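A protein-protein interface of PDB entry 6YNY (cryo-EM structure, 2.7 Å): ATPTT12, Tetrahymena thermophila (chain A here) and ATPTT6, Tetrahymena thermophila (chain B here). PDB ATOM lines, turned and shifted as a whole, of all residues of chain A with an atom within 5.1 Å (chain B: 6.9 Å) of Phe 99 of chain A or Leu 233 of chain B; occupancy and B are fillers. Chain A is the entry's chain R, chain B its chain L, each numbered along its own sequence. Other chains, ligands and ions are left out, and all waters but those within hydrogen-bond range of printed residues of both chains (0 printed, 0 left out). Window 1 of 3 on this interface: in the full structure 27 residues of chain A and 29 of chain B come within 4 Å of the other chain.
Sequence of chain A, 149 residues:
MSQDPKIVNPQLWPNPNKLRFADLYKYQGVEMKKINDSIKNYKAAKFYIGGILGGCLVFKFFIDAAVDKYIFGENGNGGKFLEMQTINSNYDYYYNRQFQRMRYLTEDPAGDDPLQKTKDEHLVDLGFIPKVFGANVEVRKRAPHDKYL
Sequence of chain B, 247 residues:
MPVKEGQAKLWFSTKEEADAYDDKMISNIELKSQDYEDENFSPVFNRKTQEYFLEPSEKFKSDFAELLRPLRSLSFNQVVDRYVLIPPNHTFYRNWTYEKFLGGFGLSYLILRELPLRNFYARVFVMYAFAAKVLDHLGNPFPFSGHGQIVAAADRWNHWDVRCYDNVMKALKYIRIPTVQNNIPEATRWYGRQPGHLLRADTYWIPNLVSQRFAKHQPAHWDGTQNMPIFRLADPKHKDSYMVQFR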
ATOM      1  N   TYR A  95       6.660 -16.523  -7.576  1.00  0.00           N
ATOM      2  CA  TYR A  95       7.272 -16.765  -8.877  1.00  0.00           C
ATOM      3  C   TYR A  95       8.586 -16.009  -9.009  1.00  0.00           C
ATOM      4  O   TYR A  95       9.567 -16.543  -9.539  1.00  0.00           O
ATOM      5  CB  TYR A  95       6.302 -16.360  -9.986  1.00  0.00           C
ATOM      6  CG  TYR A  95       6.900 -16.318 -11.373  1.00  0.00           C
ATOM      7  CD1 TYR A  95       6.796 -17.399 -12.228  1.00  0.00           C
ATOM      8  CD2 TYR A  95       7.554 -15.187 -11.831  1.00  0.00           C
ATOM      9  CE1 TYR A  95       7.334 -17.357 -13.491  1.00  0.00           C
ATOM     10  CE2 TYR A  95       8.097 -15.140 -13.089  1.00  0.00           C
ATOM     11  CZ  TYR A  95       7.983 -16.225 -13.917  1.00  0.00           C
ATOM     12  OH  TYR A  95       8.524 -16.180 -15.177  1.00  0.00           O
ATOM     13  N   ASN A  96       8.625 -14.767  -8.527  1.00  0.00           N
ATOM     14  CA  ASN A  96       9.841 -13.971  -8.628  1.00  0.00           C
ATOM     15  C   ASN A  96      10.951 -14.535  -7.755  1.00  0.00           C
ATOM     16  O   ASN A  96      12.122 -14.514  -8.143  1.00  0.00           O
ATOM     17  CB  ASN A  96       9.545 -12.524  -8.256  1.00  0.00           C
ATOM     18  CG  ASN A  96       8.616 -11.857  -9.235  1.00  0.00           C
ATOM     19  OD1 ASN A  96       8.404 -12.348 -10.339  1.00  0.00           O
ATOM     20  ND2 ASN A  96       8.063 -10.725  -8.842  1.00  0.00           N
ATOM     21  N   ARG A  97      10.607 -15.038  -6.570  1.00  0.00           N
ATOM     22  CA  ARG A  97      11.610 -15.669  -5.724  1.00  0.00           C
ATOM     23  C   ARG A  97      12.231 -16.870  -6.420  1.00  0.00           C
ATOM     24  O   ARG A  97      13.458 -16.999  -6.485  1.00  0.00           O
ATOM     25  CB  ARG A  97      10.984 -16.082  -4.395  1.00  0.00           C
ATOM     26  CG  ARG A  97      10.747 -14.946  -3.432  1.00  0.00           C
ATOM     27  CD  ARG A  97      12.048 -14.318  -2.998  1.00  0.00           C
ATOM     28  NE  ARG A  97      11.892 -13.463  -1.831  1.00  0.00           N
ATOM     29  CZ  ARG A  97      12.816 -12.613  -1.399  1.00  0.00           C
ATOM     30  NH1 ARG A  97      13.965 -12.493  -2.041  1.00  0.00           N
ATOM     31  NH2 ARG A  97      12.592 -11.877  -0.328  1.00  0.00           N
ATOM     32  N   GLN A  98      11.396 -17.762  -6.950  1.00  0.00           N
ATOM     33  CA  GLN A  98      11.917 -18.906  -7.684  1.00  0.00           C
ATOM     34  C   GLN A  98      12.658 -18.466  -8.937  1.00  0.00           C
ATOM     35  O   GLN A  98      13.577 -19.157  -9.390  1.00  0.00           O
ATOM     36  CB  GLN A  98      10.780 -19.857  -8.040  1.00  0.00           C
ATOM     37  CG  GLN A  98      11.236 -21.175  -8.617  1.00  0.00           C
ATOM     38  CD  GLN A  98      12.063 -21.978  -7.648  1.00  0.00           C
ATOM     39  OE1 GLN A  98      12.083 -21.702  -6.451  1.00  0.00           O
ATOM     40  NE2 GLN A  98      12.760 -22.978  -8.161  1.00  0.00           N
ATOM     41  N   PHE A  99      12.273 -17.329  -9.511  1.00  0.00           N
ATOM     42  CA  PHE A  99      13.029 -16.768 -10.623  1.00  0.00           C
ATOM     43  C   PHE A  99      14.408 -16.311 -10.166  1.00  0.00           C
ATOM     44  O   PHE A  99      15.385 -16.421 -10.915  1.00  0.00           O
ATOM     45  CB  PHE A  99      12.251 -15.610 -11.243  1.00  0.00           C
ATOM     46  CG  PHE A  99      12.712 -15.234 -12.611  1.00  0.00           C
ATOM     47  CD1 PHE A  99      12.030 -15.678 -13.723  1.00  0.00           C
ATOM     48  CD2 PHE A  99      13.822 -14.435 -12.791  1.00  0.00           C
ATOM     49  CE1 PHE A  99      12.444 -15.336 -14.981  1.00  0.00           C
ATOM     50  CE2 PHE A  99      14.238 -14.092 -14.049  1.00  0.00           C
ATOM     51  CZ  PHE A  99      13.549 -14.543 -15.146  1.00  0.00           C
ATOM     52  N   GLN A 100      14.505 -15.796  -8.939  1.00  0.00           N
ATOM     53  CA  GLN A 100      15.804 -15.434  -8.387  1.00  0.00           C
ATOM     54  C   GLN A 100      16.651 -16.669  -8.117  1.00  0.00           C
ATOM     55  O   GLN A 100      17.852 -16.681  -8.410  1.00  0.00           O
ATOM     56  CB  GLN A 100      15.620 -14.630  -7.103  1.00  0.00           C
ATOM     57  CG  GLN A 100      15.001 -13.265  -7.288  1.00  0.00           C
ATOM     58  CD  GLN A 100      14.669 -12.598  -5.976  1.00  0.00           C
ATOM     59  OE1 GLN A 100      14.246 -13.248  -5.027  1.00  0.00           O
ATOM     60  NE2 GLN A 100      14.870 -11.295  -5.912  1.00  0.00           N
ATOM     61  N   ARG A 101      16.048 -17.713  -7.548  1.00  0.00           N
ATOM     62  CA  ARG A 101      16.780 -18.952  -7.323  1.00  0.00           C
ATOM     63  C   ARG A 101      17.233 -19.571  -8.635  1.00  0.00           C
ATOM     64  O   ARG A 101      18.315 -20.163  -8.711  1.00  0.00           O
ATOM     65  CB  ARG A 101      15.912 -19.941  -6.548  1.00  0.00           C
ATOM     66  CG  ARG A 101      15.387 -19.415  -5.238  1.00  0.00           C
ATOM     67  CD  ARG A 101      14.702 -20.496  -4.425  1.00  0.00           C
ATOM     68  NE  ARG A 101      13.959 -19.935  -3.302  1.00  0.00           N
ATOM     69  CZ  ARG A 101      12.657 -19.674  -3.309  1.00  0.00           C
ATOM     70  NH1 ARG A 101      11.919 -19.924  -4.378  1.00  0.00           N
ATOM     71  NH2 ARG A 101      12.089 -19.158  -2.232  1.00  0.00           N
ATOM     72  N   MET A 102      16.419 -19.444  -9.681  1.00  0.00           N
ATOM     73  CA  MET A 102      16.776 -20.022 -10.967  1.00  0.00           C
ATOM     74  C   MET A 102      17.985 -19.324 -11.574  1.00  0.00           C
ATOM     75  O   MET A 102      18.844 -19.976 -12.175  1.00  0.00           O
ATOM     76  CB  MET A 102      15.577 -19.954 -11.909  1.00  0.00           C
ATOM     77  CG  MET A 102      15.829 -20.478 -13.306  1.00  0.00           C
ATOM     78  SD  MET A 102      16.480 -19.236 -14.431  1.00  0.00           S
ATOM     79  CE  MET A 102      15.097 -18.109 -14.503  1.00  0.00           C
ATOM     80  N   ARG A 103      18.073 -18.001 -11.433  1.00  0.00           N
ATOM     81  CA  ARG A 103      19.220 -17.291 -11.981  1.00  0.00           C
ATOM     82  C   ARG A 103      20.457 -17.457 -11.112  1.00  0.00           C
ATOM     83  O   ARG A 103      21.579 -17.368 -11.619  1.00  0.00           O
ATOM     84  CB  ARG A 103      18.898 -15.808 -12.168  1.00  0.00           C
ATOM     85  CG  ARG A 103      17.919 -15.510 -13.291  1.00  0.00           C
ATOM     86  CD  ARG A 103      18.353 -16.119 -14.605  1.00  0.00           C
ATOM     87  NE  ARG A 103      17.512 -15.703 -15.720  1.00  0.00           N
ATOM     88  CZ  ARG A 103      17.377 -16.394 -16.846  1.00  0.00           C
ATOM     89  NH1 ARG A 103      18.020 -17.540 -17.010  1.00  0.00           N
ATOM     90  NH2 ARG A 103      16.592 -15.943 -17.809  1.00  0.00           N
ATOM     91  N   ARG B 193      23.397 -11.900 -14.236  1.00  0.00           N
ATOM     92  CA  ARG B 193      22.117 -12.572 -14.403  1.00  0.00           C
ATOM     93  C   ARG B 193      21.203 -12.422 -13.200  1.00  0.00           C
ATOM     94  O   ARG B 193      19.995 -12.638 -13.332  1.00  0.00           O
ATOM     95  CB  ARG B 193      22.335 -14.055 -14.688  1.00  0.00           C
ATOM     96  CG  ARG B 193      23.110 -14.303 -15.943  1.00  0.00           C
ATOM     97  CD  ARG B 193      23.146 -15.767 -16.303  1.00  0.00           C
ATOM     98  NE  ARG B 193      24.391 -16.119 -16.979  1.00  0.00           N
ATOM     99  CZ  ARG B 193      25.416 -16.738 -16.404  1.00  0.00           C
ATOM    100  NH1 ARG B 193      26.500 -17.000 -17.111  1.00  0.00           N
ATOM    101  NH2 ARG B 193      25.363 -17.112 -15.137  1.00  0.00           N
ATOM    102  N   GLN B 194      21.742 -12.067 -12.042  1.00  0.00           N
ATOM    103  CA  GLN B 194      20.900 -11.805 -10.886  1.00  0.00           C
ATOM    104  C   GLN B 194      19.974 -10.654 -11.253  1.00  0.00           C
ATOM    105  O   GLN B 194      20.423  -9.507 -11.358  1.00  0.00           O
ATOM    106  CB  GLN B 194      21.738 -11.471  -9.657  1.00  0.00           C
ATOM    107  CG  GLN B 194      22.846 -12.462  -9.375  1.00  0.00           C
ATOM    108  CD  GLN B 194      22.347 -13.884  -9.269  1.00  0.00           C
ATOM    109  OE1 GLN B 194      21.494 -14.199  -8.442  1.00  0.00           O
ATOM    110  NE2 GLN B 194      22.872 -14.751 -10.116  1.00  0.00           N
ATOM    111  N   PRO B 195      18.684 -10.912 -11.447  1.00  0.00           N
ATOM    112  CA  PRO B 195      17.832  -9.913 -12.095  1.00  0.00           C
ATOM    113  C   PRO B 195      17.620  -8.680 -11.237  1.00  0.00           C
ATOM    114  O   PRO B 195      17.428  -8.763 -10.022  1.00  0.00           O
ATOM    115  CB  PRO B 195      16.523 -10.669 -12.322  1.00  0.00           C
ATOM    116  CG  PRO B 195      16.503 -11.695 -11.269  1.00  0.00           C
ATOM    117  CD  PRO B 195      17.918 -12.103 -11.049  1.00  0.00           C
ATOM    118  N   GLY B 196      17.662  -7.525 -11.892  1.00  0.00           N
ATOM    119  CA  GLY B 196      17.322  -6.285 -11.240  1.00  0.00           C
ATOM    120  C   GLY B 196      15.827  -6.082 -11.152  1.00  0.00           C
ATOM    121  O   GLY B 196      15.029  -6.835 -11.703  1.00  0.00           O
ATOM    122  N   HIS B 197      15.446  -5.031 -10.439  1.00  0.00           N
ATOM    123  CA  HIS B 197      14.048  -4.748 -10.155  1.00  0.00           C
ATOM    124  C   HIS B 197      13.497  -3.763 -11.174  1.00  0.00           C
ATOM    125  O   HIS B 197      14.111  -2.727 -11.443  1.00  0.00           O
ATOM    126  CB  HIS B 197      13.887  -4.204  -8.738  1.00  0.00           C
ATOM    127  CG  HIS B 197      14.387  -5.136  -7.685  1.00  0.00           C
ATOM    128  ND1 HIS B 197      13.696  -6.261  -7.296  1.00  0.00           N
ATOM    129  CD2 HIS B 197      15.520  -5.117  -6.945  1.00  0.00           C
ATOM    130  CE1 HIS B 197      14.380  -6.892  -6.359  1.00  0.00           C
ATOM    131  NE2 HIS B 197      15.489  -6.218  -6.127  1.00  0.00           N
ATOM    132  N   LEU B 198      12.339  -4.094 -11.732  1.00  0.00           N
ATOM    133  CA  LEU B 198      11.683  -3.293 -12.750  1.00  0.00           C
ATOM    134  C   LEU B 198      10.274  -2.964 -12.286  1.00  0.00           C
ATOM    135  O   LEU B 198       9.541  -3.849 -11.836  1.00  0.00           O
ATOM    136  CB  LEU B 198      11.663  -4.040 -14.082  1.00  0.00           C
ATOM    137  CG  LEU B 198      11.105  -3.329 -15.309  1.00  0.00           C
ATOM    138  CD1 LEU B 198      11.948  -2.142 -15.672  1.00  0.00           C
ATOM    139  CD2 LEU B 198      11.034  -4.296 -16.461  1.00  0.00           C
ATOM    140  N   LEU B 199       9.902  -1.693 -12.391  1.00  0.00           N
ATOM    141  CA  LEU B 199       8.617  -1.242 -11.881  1.00  0.00           C
ATOM    142  C   LEU B 199       7.468  -1.886 -12.647  1.00  0.00           C
ATOM    143  O   LEU B 199       7.552  -2.134 -13.851  1.00  0.00           O
ATOM    144  CB  LEU B 199       8.520   0.280 -11.974  1.00  0.00           C
ATOM    145  CG  LEU B 199       9.490   1.063 -11.095  1.00  0.00           C
ATOM    146  CD1 LEU B 199       9.447   2.530 -11.437  1.00  0.00           C
ATOM    147  CD2 LEU B 199       9.169   0.860  -9.636  1.00  0.00           C
ATOM    148  N   ARG B 200       6.380  -2.159 -11.923  1.00  0.00           N
ATOM    149  CA  ARG B 200       5.179  -2.684 -12.564  1.00  0.00           C
ATOM    150  C   ARG B 200       4.454  -1.603 -13.351  1.00  0.00           C
ATOM    151  O   ARG B 200       3.877  -1.880 -14.408  1.00  0.00           O
ATOM    152  CB  ARG B 200       4.237  -3.279 -11.519  1.00  0.00           C
ATOM    153  CG  ARG B 200       4.740  -4.522 -10.829  1.00  0.00           C
ATOM    154  CD  ARG B 200       4.890  -5.680 -11.782  1.00  0.00           C
ATOM    155  NE  ARG B 200       3.668  -5.969 -12.526  1.00  0.00           N
ATOM    156  CZ  ARG B 200       2.711  -6.795 -12.118  1.00  0.00           C
ATOM    157  NH1 ARG B 200       1.645  -6.991 -12.873  1.00  0.00           N
ATOM    158  NH2 ARG B 200       2.813  -7.427 -10.960  1.00  0.00           N
ATOM    159  N   ASN B 227      15.989  -7.595  -1.043  1.00  0.00           N
ATOM    160  CA  ASN B 227      15.770  -8.075  -2.400  1.00  0.00           C
ATOM    161  C   ASN B 227      14.318  -8.476  -2.636  1.00  0.00           C
ATOM    162  O   ASN B 227      14.039  -9.251  -3.552  1.00  0.00           O
ATOM    163  CB  ASN B 227      16.689  -9.258  -2.691  1.00  0.00           C
ATOM    164  CG  ASN B 227      16.540 -10.368  -1.681  1.00  0.00           C
ATOM    165  OD1 ASN B 227      15.618 -10.366  -0.870  1.00  0.00           O
ATOM    166  ND2 ASN B 227      17.446 -11.326  -1.726  1.00  0.00           N
ATOM    167  N   PRO B 229      11.129  -8.973  -4.168  1.00  0.00           N
ATOM    168  CA  PRO B 229      10.627  -8.678  -5.522  1.00  0.00           C
ATOM    169  C   PRO B 229       9.170  -8.233  -5.513  1.00  0.00           C
ATOM    170  O   PRO B 229       8.255  -8.928  -5.961  1.00  0.00           O
ATOM    171  CB  PRO B 229      10.845 -10.008  -6.243  1.00  0.00           C
ATOM    172  CG  PRO B 229      10.720 -11.018  -5.198  1.00  0.00           C
ATOM    173  CD  PRO B 229      11.248 -10.420  -3.940  1.00  0.00           C
ATOM    174  N   PHE B 231       8.135  -5.776  -7.231  1.00  0.00           N
ATOM    175  CA  PHE B 231       7.858  -5.404  -8.607  1.00  0.00           C
ATOM    176  C   PHE B 231       8.256  -6.570  -9.504  1.00  0.00           C
ATOM    177  O   PHE B 231       8.600  -7.656  -9.034  1.00  0.00           O
ATOM    178  CB  PHE B 231       8.607  -4.132  -9.004  1.00  0.00           C
ATOM    179  CG  PHE B 231       8.529  -3.037  -7.992  1.00  0.00           C
ATOM    180  CD1 PHE B 231       7.318  -2.481  -7.642  1.00  0.00           C
ATOM    181  CD2 PHE B 231       9.677  -2.549  -7.403  1.00  0.00           C
ATOM    182  CE1 PHE B 231       7.254  -1.472  -6.715  1.00  0.00           C
ATOM    183  CE2 PHE B 231       9.617  -1.541  -6.480  1.00  0.00           C
ATOM    184  CZ  PHE B 231       8.407  -1.002  -6.135  1.00  0.00           C
ATOM    185  N   ARG B 232       8.197  -6.341 -10.807  1.00  0.00           N
ATOM    186  CA  ARG B 232       8.697  -7.326 -11.745  1.00  0.00           C
ATOM    187  C   ARG B 232      10.214  -7.216 -11.852  1.00  0.00           C
ATOM    188  O   ARG B 232      10.842  -6.307 -11.305  1.00  0.00           O
ATOM    189  CB  ARG B 232       8.036  -7.152 -13.110  1.00  0.00           C
ATOM    190  CG  ARG B 232       8.141  -5.770 -13.688  1.00  0.00           C
ATOM    191  CD  ARG B 232       7.506  -5.713 -15.041  1.00  0.00           C
ATOM    192  NE  ARG B 232       7.540  -4.371 -15.602  1.00  0.00           N
ATOM    193  CZ  ARG B 232       7.195  -4.078 -16.849  1.00  0.00           C
ATOM    194  NH1 ARG B 232       6.799  -5.031 -17.672  1.00  0.00           N
ATOM    195  NH2 ARG B 232       7.256  -2.829 -17.272  1.00  0.00           N
ATOM    196  N   LEU B 233      10.805  -8.169 -12.560  1.00  0.00           N
ATOM    197  CA  LEU B 233      12.248  -8.286 -12.673  1.00  0.00           C
ATOM    198  C   LEU B 233      12.697  -7.962 -14.090  1.00  0.00           C
ATOM    199  O   LEU B 233      12.007  -8.283 -15.061  1.00  0.00           O
ATOM    200  CB  LEU B 233      12.703  -9.690 -12.282  1.00  0.00           C
ATOM    201  CG  LEU B 233      12.510 -10.039 -10.807  1.00  0.00           C
ATOM    202  CD1 LEU B 233      12.775 -11.505 -10.575  1.00  0.00           C
ATOM    203  CD2 LEU B 233      13.405  -9.190  -9.924  1.00  0.00           C
ATOM    204  N   ALA B 234      13.861  -7.323 -14.198  1.00  0.00           N
ATOM    205  CA  ALA B 234      14.403  -6.887 -15.482  1.00  0.00           C
ATOM    206  C   ALA B 234      15.132  -8.052 -16.149  1.00  0.00           C
ATOM    207  O   ALA B 234      16.356  -8.077 -16.290  1.00  0.00           O
ATOM    208  CB  ALA B 234      15.321  -5.690 -15.294  1.00  0.00           C
ATOM    209  N   ASP B 235      14.339  -9.039 -16.568  1.00  0.00           N
ATOM    210  CA  ASP B 235      14.850 -10.192 -17.279  1.00  0.00           C
ATOM    211  C   ASP B 235      13.922 -10.460 -18.460  1.00  0.00           C
ATOM    212  O   ASP B 235      12.691 -10.440 -18.292  1.00  0.00           O
ATOM    213  CB  ASP B 235      14.935 -11.419 -16.371  1.00  0.00           C
ATOM    214  CG  ASP B 235      15.717 -12.556 -16.995  1.00  0.00           C
ATOM    215  OD1 ASP B 235      16.948 -12.612 -16.796  1.00  0.00           O
ATOM    216  OD2 ASP B 235      15.106 -13.392 -17.689  1.00  0.00           O
ATOM    217  N   PRO B 236      14.466 -10.705 -19.654  1.00  0.00           N
ATOM    218  CA  PRO B 236      13.598 -10.927 -20.821  1.00  0.00           C
ATOM    219  C   PRO B 236      12.646 -12.095 -20.665  1.00  0.00           C
ATOM    220  O   PRO B 236      11.595 -12.116 -21.315  1.00  0.00           O
ATOM    221  CB  PRO B 236      14.598 -11.174 -21.956  1.00  0.00           C
ATOM    222  CG  PRO B 236      15.866 -10.618 -21.492  1.00  0.00           C
ATOM    223  CD  PRO B 236      15.889 -10.748 -20.017  1.00  0.00           C
ATOM    224  N   LYS B 237      12.980 -13.068 -19.827  1.00  0.00           N
ATOM    225  CA  LYS B 237      12.188 -14.278 -19.678  1.00  0.00           C
ATOM    226  C   LYS B 237      11.189 -14.202 -18.534  1.00  0.00           C
ATOM    227  O   LYS B 237      10.505 -15.192 -18.261  1.00  0.00           O
ATOM    228  CB  LYS B 237      13.116 -15.476 -19.481  1.00  0.00           C
ATOM    229  CG  LYS B 237      13.585 -16.121 -20.768  1.00  0.00           C
ATOM    230  CD  LYS B 237      14.190 -15.119 -21.724  1.00  0.00           C
ATOM    231  CE  LYS B 237      14.636 -15.782 -23.006  1.00  0.00           C
ATOM    232  NZ  LYS B 237      15.104 -14.796 -24.006  1.00  0.00           N
ATOM    233  N   HIS B 238      11.091 -13.061 -17.865  1.00  0.00           N
ATOM    234  CA  HIS B 238      10.099 -12.888 -16.817  1.00  0.00           C
ATOM    235  C   HIS B 238       8.704 -12.794 -17.421  1.00  0.00           C
ATOM    236  O   HIS B 238       8.500 -12.156 -18.456  1.00  0.00           O
ATOM    237  CB  HIS B 238      10.415 -11.636 -16.007  1.00  0.00           C
ATOM    238  CG  HIS B 238       9.700 -11.564 -14.699  1.00  0.00           C
ATOM    239  ND1 HIS B 238       8.544 -10.836 -14.522  1.00  0.00           N
ATOM    240  CD2 HIS B 238       9.981 -12.119 -13.498  1.00  0.00           C
ATOM    241  CE1 HIS B 238       8.141 -10.953 -13.270  1.00  0.00           C
ATOM    242  NE2 HIS B 238       8.997 -11.726 -12.628  1.00  0.00           N
ATOM    243  N   LYS B 239       7.740 -13.440 -16.766  1.00  0.00           N
ATOM    244  CA  LYS B 239       6.379 -13.506 -17.284  1.00  0.00           C
ATOM    245  C   LYS B 239       5.686 -12.152 -17.318  1.00  0.00           C
ATOM    246  O   LYS B 239       4.639 -12.031 -17.959  1.00  0.00           O
ATOM    247  CB  LYS B 239       5.549 -14.475 -16.446  1.00  0.00           C
ATOM    248  CG  LYS B 239       5.274 -13.993 -15.040  1.00  0.00           C
ATOM    249  CD  LYS B 239       4.480 -15.010 -14.254  1.00  0.00           C
ATOM    250  CE  LYS B 239       4.109 -14.478 -12.891  1.00  0.00           C
ATOM    251  NZ  LYS B 239       3.218 -13.307 -12.987  1.00  0.00           N
ATOM    252  N   ASP B 240       6.228 -11.144 -16.639  1.00  0.00           N
ATOM    253  CA  ASP B 240       5.663  -9.803 -16.635  1.00  0.00           C
ATOM    254  C   ASP B 240       6.559  -8.798 -17.341  1.00  0.00           C
ATOM    255  O   ASP B 240       6.307  -7.593 -17.260  1.00  0.00           O
ATOM    256  CB  ASP B 240       5.394  -9.350 -15.200  1.00  0.00           C
ATOM    257  CG  ASP B 240       4.236 -10.086 -14.563  1.00  0.00           C
ATOM    258  OD1 ASP B 240       3.232 -10.337 -15.259  1.00  0.00           O
ATOM    259  OD2 ASP B 240       4.328 -10.412 -13.363  1.00  0.00           O
ATOM    260  N   SER B 241       7.599  -9.265 -18.033  1.00  0.00           N
ATOM    261  CA  SER B 241       8.514  -8.389 -18.747  1.00  0.00           C
ATOM    262  C   SER B 241       8.816  -8.886 -20.154  1.00  0.00           C
ATOM    263  O   SER B 241       9.666  -8.301 -20.832  1.00  0.00           O
ATOM    264  CB  SER B 241       9.821  -8.236 -17.967  1.00  0.00           C
ATOM    265  OG  SER B 241       9.580  -7.827 -16.638  1.00  0.00           O
ATOM    266  N   PHE B 246      14.803  -6.232 -24.885  1.00  0.00           N
ATOM    267  CA  PHE B 246      16.135  -6.117 -24.305  1.00  0.00           C
ATOM    268  C   PHE B 246      17.160  -6.263 -25.423  1.00  0.00           C
ATOM    269  O   PHE B 246      17.393  -7.370 -25.918  1.00  0.00           O
ATOM    270  CB  PHE B 246      16.342  -7.174 -23.223  1.00  0.00           C
ATOM    271  CG  PHE B 246      15.411  -7.040 -22.058  1.00  0.00           C
ATOM    272  CD1 PHE B 246      15.867  -6.561 -20.850  1.00  0.00           C
ATOM    273  CD2 PHE B 246      14.083  -7.395 -22.168  1.00  0.00           C
ATOM    274  CE1 PHE B 246      15.017  -6.437 -19.779  1.00  0.00           C
ATOM    275  CE2 PHE B 246      13.234  -7.269 -21.097  1.00  0.00           C
ATOM    276  CZ  PHE B 246      13.701  -6.792 -19.904  1.00  0.00           C
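Of chain B, only Leu 233 (3.8 Å), Asp 235 (3.2 Å), Lys 237 (3.8 Å) and His 238 (3.9 Å) come within 4 Å of Phe 99 of chain A.
Of chain A, only Asn 96 and Phe 99 come within 4 Å of Leu 233 of chain B.
Of the printed residues of chain B, Asn 96 of chain A touches Pro 229 (3.4 Å), Phe 231 (3.1 Å), Leu 233 (3.9 Å) and His 238 (2.4 Å).
Printed residues of chain B within 4 Å of Arg 97 of chain A: Asn 227 and Pro 229.
Of the printed residues of chain A, Asp 235 of chain B touches Phe 99 (3.2 Å) and Arg 103 (3.0 Å).
Pro 236 of chain B touches none of the printed residues of chain A.
The nearest residue of chain B that does not touch Phe 99 of chain A is Pro 195 of chain B (4.1 Å).
The nearest residue of chain A that does not touch Leu 233 of chain B is Gln 100 of chain A (4.3 Å).
The nearest printed residue of chain A that does not touch Gln 194 of chain B is Gln 100 of chain A (4.4 Å).
Tyr 95 of chain A touches Lys 237 of chain B (OH to O, 3.8 Å).
His 238 of chain B touches Tyr 95 of chain A.
O of Asn 96 of chain A touches CD1 of Leu 233 of chain B, 3.9 Å away.
CZ of Arg 97 of chain A touches CD of Pro 229 of chain B, at 3.7 Å.
CD1 of Leu 233 of chain B touches CD2 of Phe 99 of chain A, at 3.8 Å.
Asp 235 of chain B touches Phe 99 of chain A (OD2 to CZ, 3.2 Å).
O of Lys 237 of chain B touches CE1 of Phe 99 of chain A, at 3.8 Å.
Arg 103 of chain A touches Arg 193 of chain B (CG to O, 3.5 Å).
CB of Arg 103 of chain A touches CD of Pro 195 of chain B, at 3.99 Å.
CB of Lys 237 of chain B touches NH2 of Arg 103 of chain A, 3.9 Å away.
Of the 22 printed residues of chain B, 11 touch a printed residue of chain A.
Hydrophobic or aromatic side chains of chain B that line the printed part of chain A: Pro 195, Pro 229, Leu 233 and His 238.
Along chain B the printed residues that touch a printed residue of chain A span positions 193 to 239.
Of the 9 printed residues of chain A, 6 touch a printed residue of chain B.
Hydrophobic or aromatic side chains of chain A within 4 Å of the printed part of chain B: Tyr 95 and Phe 99.
Among the printed residues, 19 pairs touch across the chains.
Among the printed residues, Asp or Glu carboxylates within 4 Å of a Lys or Arg side-chain nitrogen of the other chain: Arg 103 of chain A with Asp 235 of chain B.
A ring nitrogen (ND1) of His 238 of chain B lies close to the backbone NH (N) of Asp 240 of chain B (3.2 Å).
The side-chain carboxylate of Asp 235 of chain B sits at hydrogen-bond distance from the backbone NH of Lys 237 of chain B (3.0 Å).
The guanidinium group of Arg 103 of chain A is in hydrogen-bond range of the side-chain sulfur of Met 102 of chain A (3.4 Å).
OD2 of Asp 240 of chain B is in salt-bridge range of NZ of Lys 239 of chain B (3.1 Å).
NH1 of Arg 97 of chain A sits at hydrogen-bond distance from OE1 of Gln 100 of chain A (3.1 Å).
O of Leu 233 of chain B lies within hydrogen-bond range of OG of Ser 241 of chain B.
The backbone carbonyl oxygen (O) of Phe 231 of chain B sits at hydrogen-bond distance from the side-chain amide nitrogen (ND2) of Asn 96 of chain A (3.1 Å).
NH1 of Arg 97 of chain A lies within hydrogen-bond range of OD1 of Asn 227 of chain B (2.9 Å).
O of Pro 229 of chain B lies within hydrogen-bond range of ND2 of Asn 96 of chain A.
OD1 of Asn 96 of chain A lies within hydrogen-bond range of NE2 of His 238 of chain B (2.4 Å).
The side-chain amide nitrogen (NE2) of Gln 100 of chain A sits at hydrogen-bond distance from the backbone carbonyl oxygen (O) of Asn 227 of chain B (3.2 Å).
The side-chain amide nitrogen (NE2) of Gln 194 of chain B sits at hydrogen-bond distance from the backbone carbonyl oxygen (O) of Arg 103 of chain A, at 3.3 Å.
The backbone NH of Lys 239 of chain B is in hydrogen-bond range of the side-chain hydroxyl of Tyr 95 of chain A.
The guanidinium group (NH2) of Arg 103 of chain A is in salt-bridge range of the side-chain carboxylate (OD2) of Asp 235 of chain B, at 3.0 Å.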
